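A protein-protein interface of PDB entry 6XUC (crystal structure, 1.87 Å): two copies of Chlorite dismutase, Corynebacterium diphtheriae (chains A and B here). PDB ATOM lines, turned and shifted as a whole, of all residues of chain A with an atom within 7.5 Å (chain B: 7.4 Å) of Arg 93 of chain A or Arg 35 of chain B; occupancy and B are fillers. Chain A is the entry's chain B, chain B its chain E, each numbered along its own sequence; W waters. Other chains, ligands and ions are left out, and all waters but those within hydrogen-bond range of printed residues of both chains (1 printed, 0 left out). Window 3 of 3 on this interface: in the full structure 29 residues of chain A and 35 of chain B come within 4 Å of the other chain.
The guanidinium group (NH1) of Arg 93 of chain A lies within hydrogen-bond range of the backbone carbonyl oxygen (O) of Val 234 of chain B, at 3.0 Å.
NH2 of Arg 35 of chain B lies within hydrogen-bond range of O of Pro 236 of chain B, 3.4 Å away.
The backbone carbonyl oxygen (O) of Leu 235 of chain B lies within hydrogen-bond range of the guanidinium group (NH1) of Arg 35 of chain B, at 2.8 Å.
The backbone carbonyl oxygen of Arg 93 of chain A is in hydrogen-bond range of the side-chain amide nitrogen of Gln 99 of chain A (3.4 Å).
The backbone carbonyl oxygen of Gly 32 of chain B is in hydrogen-bond range of the guanidinium group of Arg 35 of chain B.
The side-chain carboxylate of Glu 94 of chain A lies within salt-bridge range of the guanidinium group of Arg 93 of chain A, 3.1 Å away.
The guanidinium group (NH1) of Arg 35 of chain B lies within hydrogen-bond range of the backbone carbonyl oxygen (O) of Val 232 of chain B (2.8 Å).
Among the printed residues, pairs that only touch across the chains: Arg 93 of chain A with Leu 235 of chain B (3.3 Å), Arg 93 of chain A with Asn 233 of chain B (3.5 Å), Arg 92 of chain A with Pro 236 of chain B (3.5 Å), Ala 89 of chain A with Val 234 of chain B (3.7 Å) and Arg 93 of chain A with Arg 35 of chain B (3.8 Å).
Printed residues of chain B within 4 Å of Ala 89 of chain A: Val 234 (3.7 Å).
Of the printed residues of chain B, Arg 92 of chain A touches Pro 236.
Of the printed residues of chain B, Arg 93 of chain A touches Arg 35 (3.8 Å), Asn 233 (3.5 Å), Val 234 (3.0 Å) and Leu 235 (3.3 Å).
Arg 35 of chain B touches just one residue of chain A: Arg 93.
Ala 40 of chain B touches none of the printed residues of chain A.
Of the printed residues of chain A, Asn 233 of chain B touches Arg 93.
Of the printed residues of chain A, Val 234 of chain B touches Ala 89 (3.7 Å) and Arg 93 (3.0 Å).
Of the printed residues of chain A, Leu 235 of chain B touches Arg 93.
The nearest residue of chain A that does not touch Arg 35 of chain B is Glu 94 of chain A (7.4 Å).
Hydrophobic or aromatic side chains of chain A within 4 Å of the printed part of chain B: Ala 89.
Of the 18 printed residues of chain B, 5 touch a printed residue of chain A.
Among the printed residues, no Asp or Glu carboxylate lies within 4 Å of a Lys or Arg side-chain nitrogen of the other chain.
No position is printed for both chains.
Of the 6 pairs that touch across the chains among the printed residues, none has its exchanged pair printed and touching as well.
Water W1 lies within hydrogen-bond range of O of Val 234 of chain B (2.8 Å) and O of Ala 89 of chain A (2.8 Å).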
ATOM      1  N   GLN A  85     -12.436 -29.751   8.456  1.00  0.00           N
ATOM      2  CA  GLN A  85     -13.312 -28.601   8.678  1.00  0.00           C
ATOM      3  C   GLN A  85     -13.030 -27.517   7.663  1.00  0.00           C
ATOM      4  O   GLN A  85     -13.956 -26.966   7.044  1.00  0.00           O
ATOM      5  CB  GLN A  85     -13.120 -28.005  10.076  1.00  0.00           C
ATOM      6  CG  GLN A  85     -13.590 -28.802  11.234  1.00  0.00           C
ATOM      7  CD  GLN A  85     -13.522 -27.981  12.499  1.00  0.00           C
ATOM      8  OE1 GLN A  85     -12.441 -27.745  13.009  1.00  0.00           O
ATOM      9  NE2 GLN A  85     -14.674 -27.504  12.986  1.00  0.00           N
ATOM     10  N   ALA A  86     -11.745 -27.157   7.521  1.00  0.00           N
ATOM     11  CA  ALA A  86     -11.359 -26.095   6.601  1.00  0.00           C
ATOM     12  C   ALA A  86     -11.757 -26.425   5.172  1.00  0.00           C
ATOM     13  O   ALA A  86     -12.237 -25.552   4.438  1.00  0.00           O
ATOM     14  CB  ALA A  86      -9.851 -25.851   6.676  1.00  0.00           C
ATOM     15  N   ALA A  87     -11.535 -27.677   4.749  1.00  0.00           N
ATOM     16  CA  ALA A  87     -11.804 -28.036   3.359  1.00  0.00           C
ATOM     17  C   ALA A  87     -13.303 -28.110   3.090  1.00  0.00           C
ATOM     18  O   ALA A  87     -13.757 -27.690   2.021  1.00  0.00           O
ATOM     19  CB  ALA A  87     -11.130 -29.366   3.010  1.00  0.00           C
ATOM     20  N   PHE A  88     -14.062 -28.711   4.014  1.00  0.00           N
ATOM     21  CA  PHE A  88     -15.524 -28.686   3.980  1.00  0.00           C
ATOM     22  C   PHE A  88     -16.045 -27.262   3.871  1.00  0.00           C
ATOM     23  O   PHE A  88     -16.806 -26.937   2.954  1.00  0.00           O
ATOM     24  CB  PHE A  88     -16.055 -29.378   5.251  1.00  0.00           C
ATOM     25  CG  PHE A  88     -17.562 -29.281   5.451  1.00  0.00           C
ATOM     26  CD1 PHE A  88     -18.440 -30.105   4.768  1.00  0.00           C
ATOM     27  CD2 PHE A  88     -18.083 -28.369   6.321  1.00  0.00           C
ATOM     28  CE1 PHE A  88     -19.790 -30.010   4.959  1.00  0.00           C
ATOM     29  CE2 PHE A  88     -19.442 -28.261   6.500  1.00  0.00           C
ATOM     30  CZ  PHE A  88     -20.294 -29.088   5.831  1.00  0.00           C
ATOM     31  N   ALA A  89     -15.630 -26.378   4.786  1.00  0.00           N
ATOM     32  CA  ALA A  89     -16.151 -25.014   4.744  1.00  0.00           C
ATOM     33  C   ALA A  89     -15.745 -24.335   3.446  1.00  0.00           C
ATOM     34  O   ALA A  89     -16.524 -23.581   2.854  1.00  0.00           O
ATOM     35  CB  ALA A  89     -15.664 -24.212   5.953  1.00  0.00           C
ATOM     36  N   ARG A  90     -14.532 -24.612   2.970  1.00  0.00           N
ATOM     37  CA  ARG A  90     -14.068 -23.959   1.750  1.00  0.00           C
ATOM     38  C   ARG A  90     -14.827 -24.465   0.534  1.00  0.00           C
ATOM     39  O   ARG A  90     -15.165 -23.681  -0.352  1.00  0.00           O
ATOM     40  CB  ARG A  90     -12.554 -24.140   1.597  1.00  0.00           C
ATOM     41  CG  ARG A  90     -11.950 -23.617   0.289  1.00  0.00           C
ATOM     42  CD  ARG A  90     -10.407 -23.512   0.421  1.00  0.00           C
ATOM     43  NE  ARG A  90      -9.820 -24.694   1.061  1.00  0.00           N
ATOM     44  CZ  ARG A  90      -9.159 -24.702   2.226  1.00  0.00           C
ATOM     45  NH1 ARG A  90      -8.973 -23.580   2.917  1.00  0.00           N
ATOM     46  NH2 ARG A  90      -8.679 -25.851   2.702  1.00  0.00           N
ATOM     47  N   PHE A  91     -15.150 -25.754   0.492  1.00  0.00           N
ATOM     48  CA  PHE A  91     -16.032 -26.257  -0.551  1.00  0.00           C
ATOM     49  C   PHE A  91     -17.328 -25.463  -0.591  1.00  0.00           C
ATOM     50  O   PHE A  91     -17.755 -24.987  -1.640  1.00  0.00           O
ATOM     51  CB  PHE A  91     -16.334 -27.732  -0.293  1.00  0.00           C
ATOM     52  CG  PHE A  91     -17.245 -28.350  -1.318  1.00  0.00           C
ATOM     53  CD1 PHE A  91     -16.803 -28.566  -2.616  1.00  0.00           C
ATOM     54  CD2 PHE A  91     -18.543 -28.702  -0.989  1.00  0.00           C
ATOM     55  CE1 PHE A  91     -17.646 -29.147  -3.545  1.00  0.00           C
ATOM     56  CE2 PHE A  91     -19.374 -29.271  -1.909  1.00  0.00           C
ATOM     57  CZ  PHE A  91     -18.930 -29.486  -3.189  1.00  0.00           C
ATOM     58  N   ARG A  92     -17.958 -25.289   0.559  1.00  0.00           N
ATOM     59  CA  ARG A  92     -19.249 -24.614   0.583  1.00  0.00           C
ATOM     60  C   ARG A  92     -19.122 -23.141   0.241  1.00  0.00           C
ATOM     61  O   ARG A  92     -19.988 -22.571  -0.431  1.00  0.00           O
ATOM     62  CB  ARG A  92     -19.868 -24.748   1.964  1.00  0.00           C
ATOM     63  CG  ARG A  92     -20.146 -26.169   2.358  1.00  0.00           C
ATOM     64  CD  ARG A  92     -20.742 -26.232   3.745  1.00  0.00           C
ATOM     65  NE  ARG A  92     -22.040 -25.598   3.786  1.00  0.00           N
ATOM     66  CZ  ARG A  92     -22.647 -25.185   4.888  1.00  0.00           C
ATOM     67  NH1 ARG A  92     -22.064 -25.317   6.082  1.00  0.00           N
ATOM     68  NH2 ARG A  92     -23.856 -24.632   4.786  1.00  0.00           N
ATOM     69  N   ARG A  93     -18.085 -22.500   0.761  1.00  0.00           N
ATOM     70  CA  ARG A  93     -17.956 -21.056   0.667  1.00  0.00           C
ATOM     71  C   ARG A  93     -17.334 -20.617  -0.655  1.00  0.00           C
ATOM     72  O   ARG A  93     -17.657 -19.536  -1.143  1.00  0.00           O
ATOM     73  CB  ARG A  93     -17.114 -20.560   1.842  1.00  0.00           C
ATOM     74  CG  ARG A  93     -16.915 -19.056   1.940  1.00  0.00           C
ATOM     75  CD  ARG A  93     -15.928 -18.753   3.071  1.00  0.00           C
ATOM     76  NE  ARG A  93     -14.595 -19.287   2.783  1.00  0.00           N
ATOM     77  CZ  ARG A  93     -13.996 -20.299   3.416  1.00  0.00           C
ATOM     78  NH1 ARG A  93     -14.572 -20.947   4.415  1.00  0.00           N
ATOM     79  NH2 ARG A  93     -12.780 -20.669   3.047  1.00  0.00           N
ATOM     80  N   GLU A  94     -16.452 -21.420  -1.250  1.00  0.00           N
ATOM     81  CA  GLU A  94     -15.619 -20.923  -2.342  1.00  0.00           C
ATOM     82  C   GLU A  94     -15.731 -21.709  -3.645  1.00  0.00           C
ATOM     83  O   GLU A  94     -14.894 -21.518  -4.534  1.00  0.00           O
ATOM     84  CB  GLU A  94     -14.148 -20.878  -1.899  1.00  0.00           C
ATOM     85  CG  GLU A  94     -13.837 -19.770  -0.893  1.00  0.00           C
ATOM     86  CD  GLU A  94     -12.361 -19.690  -0.521  1.00  0.00           C
ATOM     87  OE1 GLU A  94     -11.509 -20.249  -1.247  1.00  0.00           O
ATOM     88  OE2 GLU A  94     -12.059 -19.066   0.511  1.00  0.00           O
ATOM     89  N   THR A  95     -16.741 -22.558  -3.809  1.00  0.00           N
ATOM     90  CA  THR A  95     -17.056 -23.122  -5.123  1.00  0.00           C
ATOM     91  C   THR A  95     -18.554 -23.004  -5.383  1.00  0.00           C
ATOM     92  O   THR A  95     -19.379 -23.114  -4.463  1.00  0.00           O
ATOM     93  CB  THR A  95     -16.650 -24.594  -5.262  1.00  0.00           C
ATOM     94  OG1 THR A  95     -17.584 -25.426  -4.554  1.00  0.00           O
ATOM     95  CG2 THR A  95     -15.272 -24.812  -4.695  1.00  0.00           C
ATOM     96  N   VAL A  96     -18.906 -22.743  -6.642  1.00  0.00           N
ATOM     97  CA  VAL A  96     -20.322 -22.658  -6.976  1.00  0.00           C
ATOM     98  C   VAL A  96     -20.997 -24.001  -6.734  1.00  0.00           C
ATOM     99  O   VAL A  96     -22.133 -24.044  -6.267  1.00  0.00           O
ATOM    100  CB  VAL A  96     -20.472 -22.141  -8.422  1.00  0.00           C
ATOM    101  CG1 VAL A  96     -21.922 -22.147  -8.864  1.00  0.00           C
ATOM    102  CG2 VAL A  96     -19.934 -20.734  -8.493  1.00  0.00           C
ATOM    103  N   GLY A  98     -20.440 -26.039  -4.294  1.00  0.00           N
ATOM    104  CA  GLY A  98     -20.807 -26.029  -2.888  1.00  0.00           C
ATOM    105  C   GLY A  98     -21.826 -24.958  -2.544  1.00  0.00           C
ATOM    106  O   GLY A  98     -22.638 -25.136  -1.637  1.00  0.00           O
ATOM    107  N   GLN A  99     -21.793 -23.843  -3.267  1.00  0.00           N
ATOM    108  CA  GLN A  99     -22.761 -22.770  -3.073  1.00  0.00           C
ATOM    109  C   GLN A  99     -24.162 -23.159  -3.512  1.00  0.00           C
ATOM    110  O   GLN A  99     -25.151 -22.681  -2.939  1.00  0.00           O
ATOM    111  CB  GLN A  99     -22.333 -21.544  -3.886  1.00  0.00           C
ATOM    112  CG  GLN A  99     -21.204 -20.743  -3.288  1.00  0.00           C
ATOM    113  CD  GLN A  99     -20.583 -19.815  -4.308  1.00  0.00           C
ATOM    114  OE1 GLN A  99     -21.109 -19.650  -5.407  1.00  0.00           O
ATOM    115  NE2 GLN A  99     -19.459 -19.210  -3.956  1.00  0.00           N
ATOM    116  N   LEU B  31     -25.023 -13.918   4.318  1.00  0.00           N
ATOM    117  CA  LEU B  31     -23.829 -13.179   4.697  1.00  0.00           C
ATOM    118  C   LEU B  31     -23.081 -12.628   3.503  1.00  0.00           C
ATOM    119  O   LEU B  31     -22.432 -11.583   3.617  1.00  0.00           O
ATOM    120  CB  LEU B  31     -22.892 -14.082   5.489  1.00  0.00           C
ATOM    121  CG  LEU B  31     -22.052 -13.424   6.575  1.00  0.00           C
ATOM    122  CD1 LEU B  31     -22.914 -12.900   7.710  1.00  0.00           C
ATOM    123  CD2 LEU B  31     -21.060 -14.467   7.054  1.00  0.00           C
ATOM    124  N   GLY B  32     -23.138 -13.326   2.374  1.00  0.00           N
ATOM    125  CA  GLY B  32     -22.450 -12.881   1.189  1.00  0.00           C
ATOM    126  C   GLY B  32     -20.958 -12.747   1.411  1.00  0.00           C
ATOM    127  O   GLY B  32     -20.353 -13.410   2.259  1.00  0.00           O
ATOM    128  N   SER B  33     -20.361 -11.851   0.635  1.00  0.00           N
ATOM    129  CA  SER B  33     -18.924 -11.657   0.604  1.00  0.00           C
ATOM    130  C   SER B  33     -18.458 -10.434   1.354  1.00  0.00           C
ATOM    131  O   SER B  33     -17.250 -10.306   1.605  1.00  0.00           O
ATOM    132  CB  SER B  33     -18.432 -11.548  -0.848  1.00  0.00           C
ATOM    133  OG  SER B  33     -17.322 -10.670  -0.961  1.00  0.00           O
ATOM    134  N   ASP B  34     -19.280  -9.487   1.731  1.00  0.00           N
ATOM    135  CA  ASP B  34     -18.752  -8.347   2.428  1.00  0.00           C
ATOM    136  C   ASP B  34     -19.172  -8.439   3.843  1.00  0.00           C
ATOM    137  O   ASP B  34     -20.197  -7.849   4.356  1.00  0.00           O
ATOM    138  CB  ASP B  34     -19.014  -7.032   1.799  1.00  0.00           C
ATOM    139  CG  ASP B  34     -20.455  -6.693   1.786  1.00  0.00           C
ATOM    140  OD1 ASP B  34     -21.254  -7.534   2.236  1.00  0.00           O
ATOM    141  OD2 ASP B  34     -20.822  -5.579   1.337  1.00  0.00           O
ATOM    142  N   ARG B  35     -18.316  -9.050   4.653  1.00  0.00           N
ATOM    143  CA  ARG B  35     -18.440  -9.479   5.983  1.00  0.00           C
ATOM    144  C   ARG B  35     -17.697  -8.591   6.958  1.00  0.00           C
ATOM    145  O   ARG B  35     -17.768  -8.848   8.156  1.00  0.00           O
ATOM    146  CB  ARG B  35     -17.883 -10.904   6.119  1.00  0.00           C
ATOM    147  CG  ARG B  35     -18.059 -11.768   4.911  1.00  0.00           C
ATOM    148  CD  ARG B  35     -17.920 -13.219   5.307  1.00  0.00           C
ATOM    149  NE  ARG B  35     -18.451 -14.092   4.277  1.00  0.00           N
ATOM    150  CZ  ARG B  35     -18.447 -15.415   4.353  1.00  0.00           C
ATOM    151  NH1 ARG B  35     -17.943 -15.996   5.426  1.00  0.00           N
ATOM    152  NH2 ARG B  35     -18.951 -16.147   3.356  1.00  0.00           N
ATOM    153  N   ALA B  36     -16.951  -7.580   6.503  1.00  0.00           N
ATOM    154  CA  ALA B  36     -16.061  -6.902   7.438  1.00  0.00           C
ATOM    155  C   ALA B  36     -16.848  -6.039   8.414  1.00  0.00           C
ATOM    156  O   ALA B  36     -16.527  -6.003   9.609  1.00  0.00           O
ATOM    157  CB  ALA B  36     -15.025  -6.069   6.678  1.00  0.00           C
ATOM    158  N   GLU B  37     -17.870  -5.324   7.926  1.00  0.00           N
ATOM    159  CA  GLU B  37     -18.758  -4.594   8.826  1.00  0.00           C
ATOM    160  C   GLU B  37     -19.538  -5.547   9.727  1.00  0.00           C
ATOM    161  O   GLU B  37     -19.789  -5.245  10.896  1.00  0.00           O
ATOM    162  CB  GLU B  37     -19.718  -3.707   8.029  1.00  0.00           C
ATOM    163  CG  GLU B  37     -19.041  -2.729   7.064  1.00  0.00           C
ATOM    164  CD  GLU B  37     -19.885  -1.488   6.799  1.00  0.00           C
ATOM    165  OE1 GLU B  37     -21.064  -1.473   7.227  1.00  0.00           O
ATOM    166  OE2 GLU B  37     -19.368  -0.531   6.170  1.00  0.00           O
ATOM    167  N   ILE B  38     -19.945  -6.701   9.199  1.00  0.00           N
ATOM    168  CA  ILE B  38     -20.657  -7.663  10.027  1.00  0.00           C
ATOM    169  C   ILE B  38     -19.777  -8.133  11.178  1.00  0.00           C
ATOM    170  O   ILE B  38     -20.230  -8.220  12.329  1.00  0.00           O
ATOM    171  CB  ILE B  38     -21.143  -8.836   9.156  1.00  0.00           C
ATOM    172  CG1 ILE B  38     -22.318  -8.375   8.308  1.00  0.00           C
ATOM    173  CG2 ILE B  38     -21.495  -9.998  10.026  1.00  0.00           C
ATOM    174  CD1 ILE B  38     -22.450  -9.110   6.981  1.00  0.00           C
ATOM    175  N   VAL B  39     -18.502  -8.430  10.885  1.00  0.00           N
ATOM    176  CA  VAL B  39     -17.556  -8.858  11.915  1.00  0.00           C
ATOM    177  C   VAL B  39     -17.341  -7.755  12.940  1.00  0.00           C
ATOM    178  O   VAL B  39     -17.360  -7.990  14.149  1.00  0.00           O
ATOM    179  CB  VAL B  39     -16.212  -9.251  11.276  1.00  0.00           C
ATOM    180  CG1 VAL B  39     -15.096  -9.296  12.336  1.00  0.00           C
ATOM    181  CG2 VAL B  39     -16.313 -10.557  10.573  1.00  0.00           C
ATOM    182  N   ALA B  40     -17.038  -6.548  12.464  1.00  0.00           N
ATOM    183  CA  ALA B  40     -16.755  -5.450  13.381  1.00  0.00           C
ATOM    184  C   ALA B  40     -17.955  -5.186  14.283  1.00  0.00           C
ATOM    185  O   ALA B  40     -17.801  -5.025  15.497  1.00  0.00           O
ATOM    186  CB  ALA B  40     -16.381  -4.191  12.596  1.00  0.00           C
ATOM    187  N   GLN B  41     -19.163  -5.139  13.698  1.00  0.00           N
ATOM    188  CA  GLN B  41     -20.375  -4.993  14.509  1.00  0.00           C
ATOM    189  C   GLN B  41     -20.507  -6.116  15.540  1.00  0.00           C
ATOM    190  O   GLN B  41     -20.849  -5.856  16.697  1.00  0.00           O
ATOM    191  CB  GLN B  41     -21.618  -4.962  13.621  1.00  0.00           C
ATOM    192  CG  GLN B  41     -22.920  -4.640  14.397  1.00  0.00           C
ATOM    193  CD  GLN B  41     -24.179  -4.688  13.529  1.00  0.00           C
ATOM    194  OE1 GLN B  41     -24.451  -5.675  12.844  1.00  0.00           O
ATOM    195  NE2 GLN B  41     -24.950  -3.616  13.562  1.00  0.00           N
ATOM    196  N   LEU B 231     -14.336 -16.955  13.239  1.00  0.00           N
ATOM    197  CA  LEU B 231     -15.534 -17.724  12.969  1.00  0.00           C
ATOM    198  C   LEU B 231     -16.257 -17.199  11.727  1.00  0.00           C
ATOM    199  O   LEU B 231     -16.606 -17.972  10.838  1.00  0.00           O
ATOM    200  CB  LEU B 231     -16.416 -17.711  14.210  1.00  0.00           C
ATOM    201  CG  LEU B 231     -17.693 -18.536  14.115  1.00  0.00           C
ATOM    202  CD1 LEU B 231     -18.804 -17.696  13.509  1.00  0.00           C
ATOM    203  CD2 LEU B 231     -17.473 -19.820  13.325  1.00  0.00           C
ATOM    204  N   VAL B 232     -16.462 -15.885  11.645  1.00  0.00           N
ATOM    205  CA  VAL B 232     -17.321 -15.398  10.566  1.00  0.00           C
ATOM    206  C   VAL B 232     -16.711 -15.614   9.175  1.00  0.00           C
ATOM    207  O   VAL B 232     -17.447 -15.734   8.184  1.00  0.00           O
ATOM    208  CB  VAL B 232     -17.641 -13.913  10.792  1.00  0.00           C
ATOM    209  CG1 VAL B 232     -18.307 -13.365   9.561  1.00  0.00           C
ATOM    210  CG2 VAL B 232     -18.479 -13.732  12.061  1.00  0.00           C
ATOM    211  N   ASN B 233     -15.376 -15.633   9.061  1.00  0.00           N
ATOM    212  CA  ASN B 233     -14.742 -15.816   7.753  1.00  0.00           C
ATOM    213  C   ASN B 233     -14.838 -17.252   7.250  1.00  0.00           C
ATOM    214  O   ASN B 233     -14.642 -17.492   6.056  1.00  0.00           O
ATOM    215  CB  ASN B 233     -13.282 -15.365   7.822  1.00  0.00           C
ATOM    216  CG  ASN B 233     -13.151 -13.859   8.061  1.00  0.00           C
ATOM    217  OD1 ASN B 233     -14.067 -13.083   7.770  1.00  0.00           O
ATOM    218  ND2 ASN B 233     -12.026 -13.450   8.613  1.00  0.00           N
ATOM    219  N   VAL B 234     -15.125 -18.199   8.138  1.00  0.00           N
ATOM    220  CA  VAL B 234     -15.350 -19.594   7.789  1.00  0.00           C
ATOM    221  C   VAL B 234     -16.702 -19.812   7.113  1.00  0.00           C
ATOM    222  O   VAL B 234     -16.858 -20.734   6.307  1.00  0.00           O
ATOM    223  CB  VAL B 234     -15.262 -20.425   9.088  1.00  0.00           C
ATOM    224  CG1 VAL B 234     -15.588 -21.885   8.833  1.00  0.00           C
ATOM    225  CG2 VAL B 234     -13.881 -20.264   9.705  1.00  0.00           C
ATOM    226  N   LEU B 235     -17.693 -18.998   7.433  1.00  0.00           N
ATOM    227  CA  LEU B 235     -19.078 -19.357   7.159  1.00  0.00           C
ATOM    228  C   LEU B 235     -19.367 -19.338   5.662  1.00  0.00           C
ATOM    229  O   LEU B 235     -18.676 -18.669   4.893  1.00  0.00           O
ATOM    230  CB  LEU B 235     -20.005 -18.392   7.896  1.00  0.00           C
ATOM    231  CG  LEU B 235     -19.893 -18.528   9.406  1.00  0.00           C
ATOM    232  CD1 LEU B 235     -20.559 -17.414  10.119  1.00  0.00           C
ATOM    233  CD2 LEU B 235     -20.504 -19.840   9.835  1.00  0.00           C
ATOM    234  N   PRO B 236     -20.396 -20.072   5.222  1.00  0.00           N
ATOM    235  CA  PRO B 236     -20.743 -20.030   3.791  1.00  0.00           C
ATOM    236  C   PRO B 236     -21.388 -18.731   3.359  1.00  0.00           C
ATOM    237  O   PRO B 236     -21.234 -18.343   2.199  1.00  0.00           O
ATOM    238  CB  PRO B 236     -21.702 -21.219   3.620  1.00  0.00           C
ATOM    239  CG  PRO B 236     -22.217 -21.499   4.942  1.00  0.00           C
ATOM    240  CD  PRO B 236     -21.215 -21.042   5.962  1.00  0.00           C
ATOM    241  N   GLY B 237     -22.121 -18.050   4.227  1.00  0.00           N
ATOM    242  CA  GLY B 237     -22.766 -16.807   3.815  1.00  0.00           C
ATOM    243  C   GLY B 237     -23.393 -16.766   2.415  1.00  0.00           C
ATOM    244  O   GLY B 237     -23.671 -15.712   1.827  1.00  0.00           O
ATOM    245  OXT GLY B 237     -23.682 -17.793   1.808  1.00  0.00           O
HETATM  246  O   HOH W   1     -18.336 -22.461   4.712  1.00  0.00           O
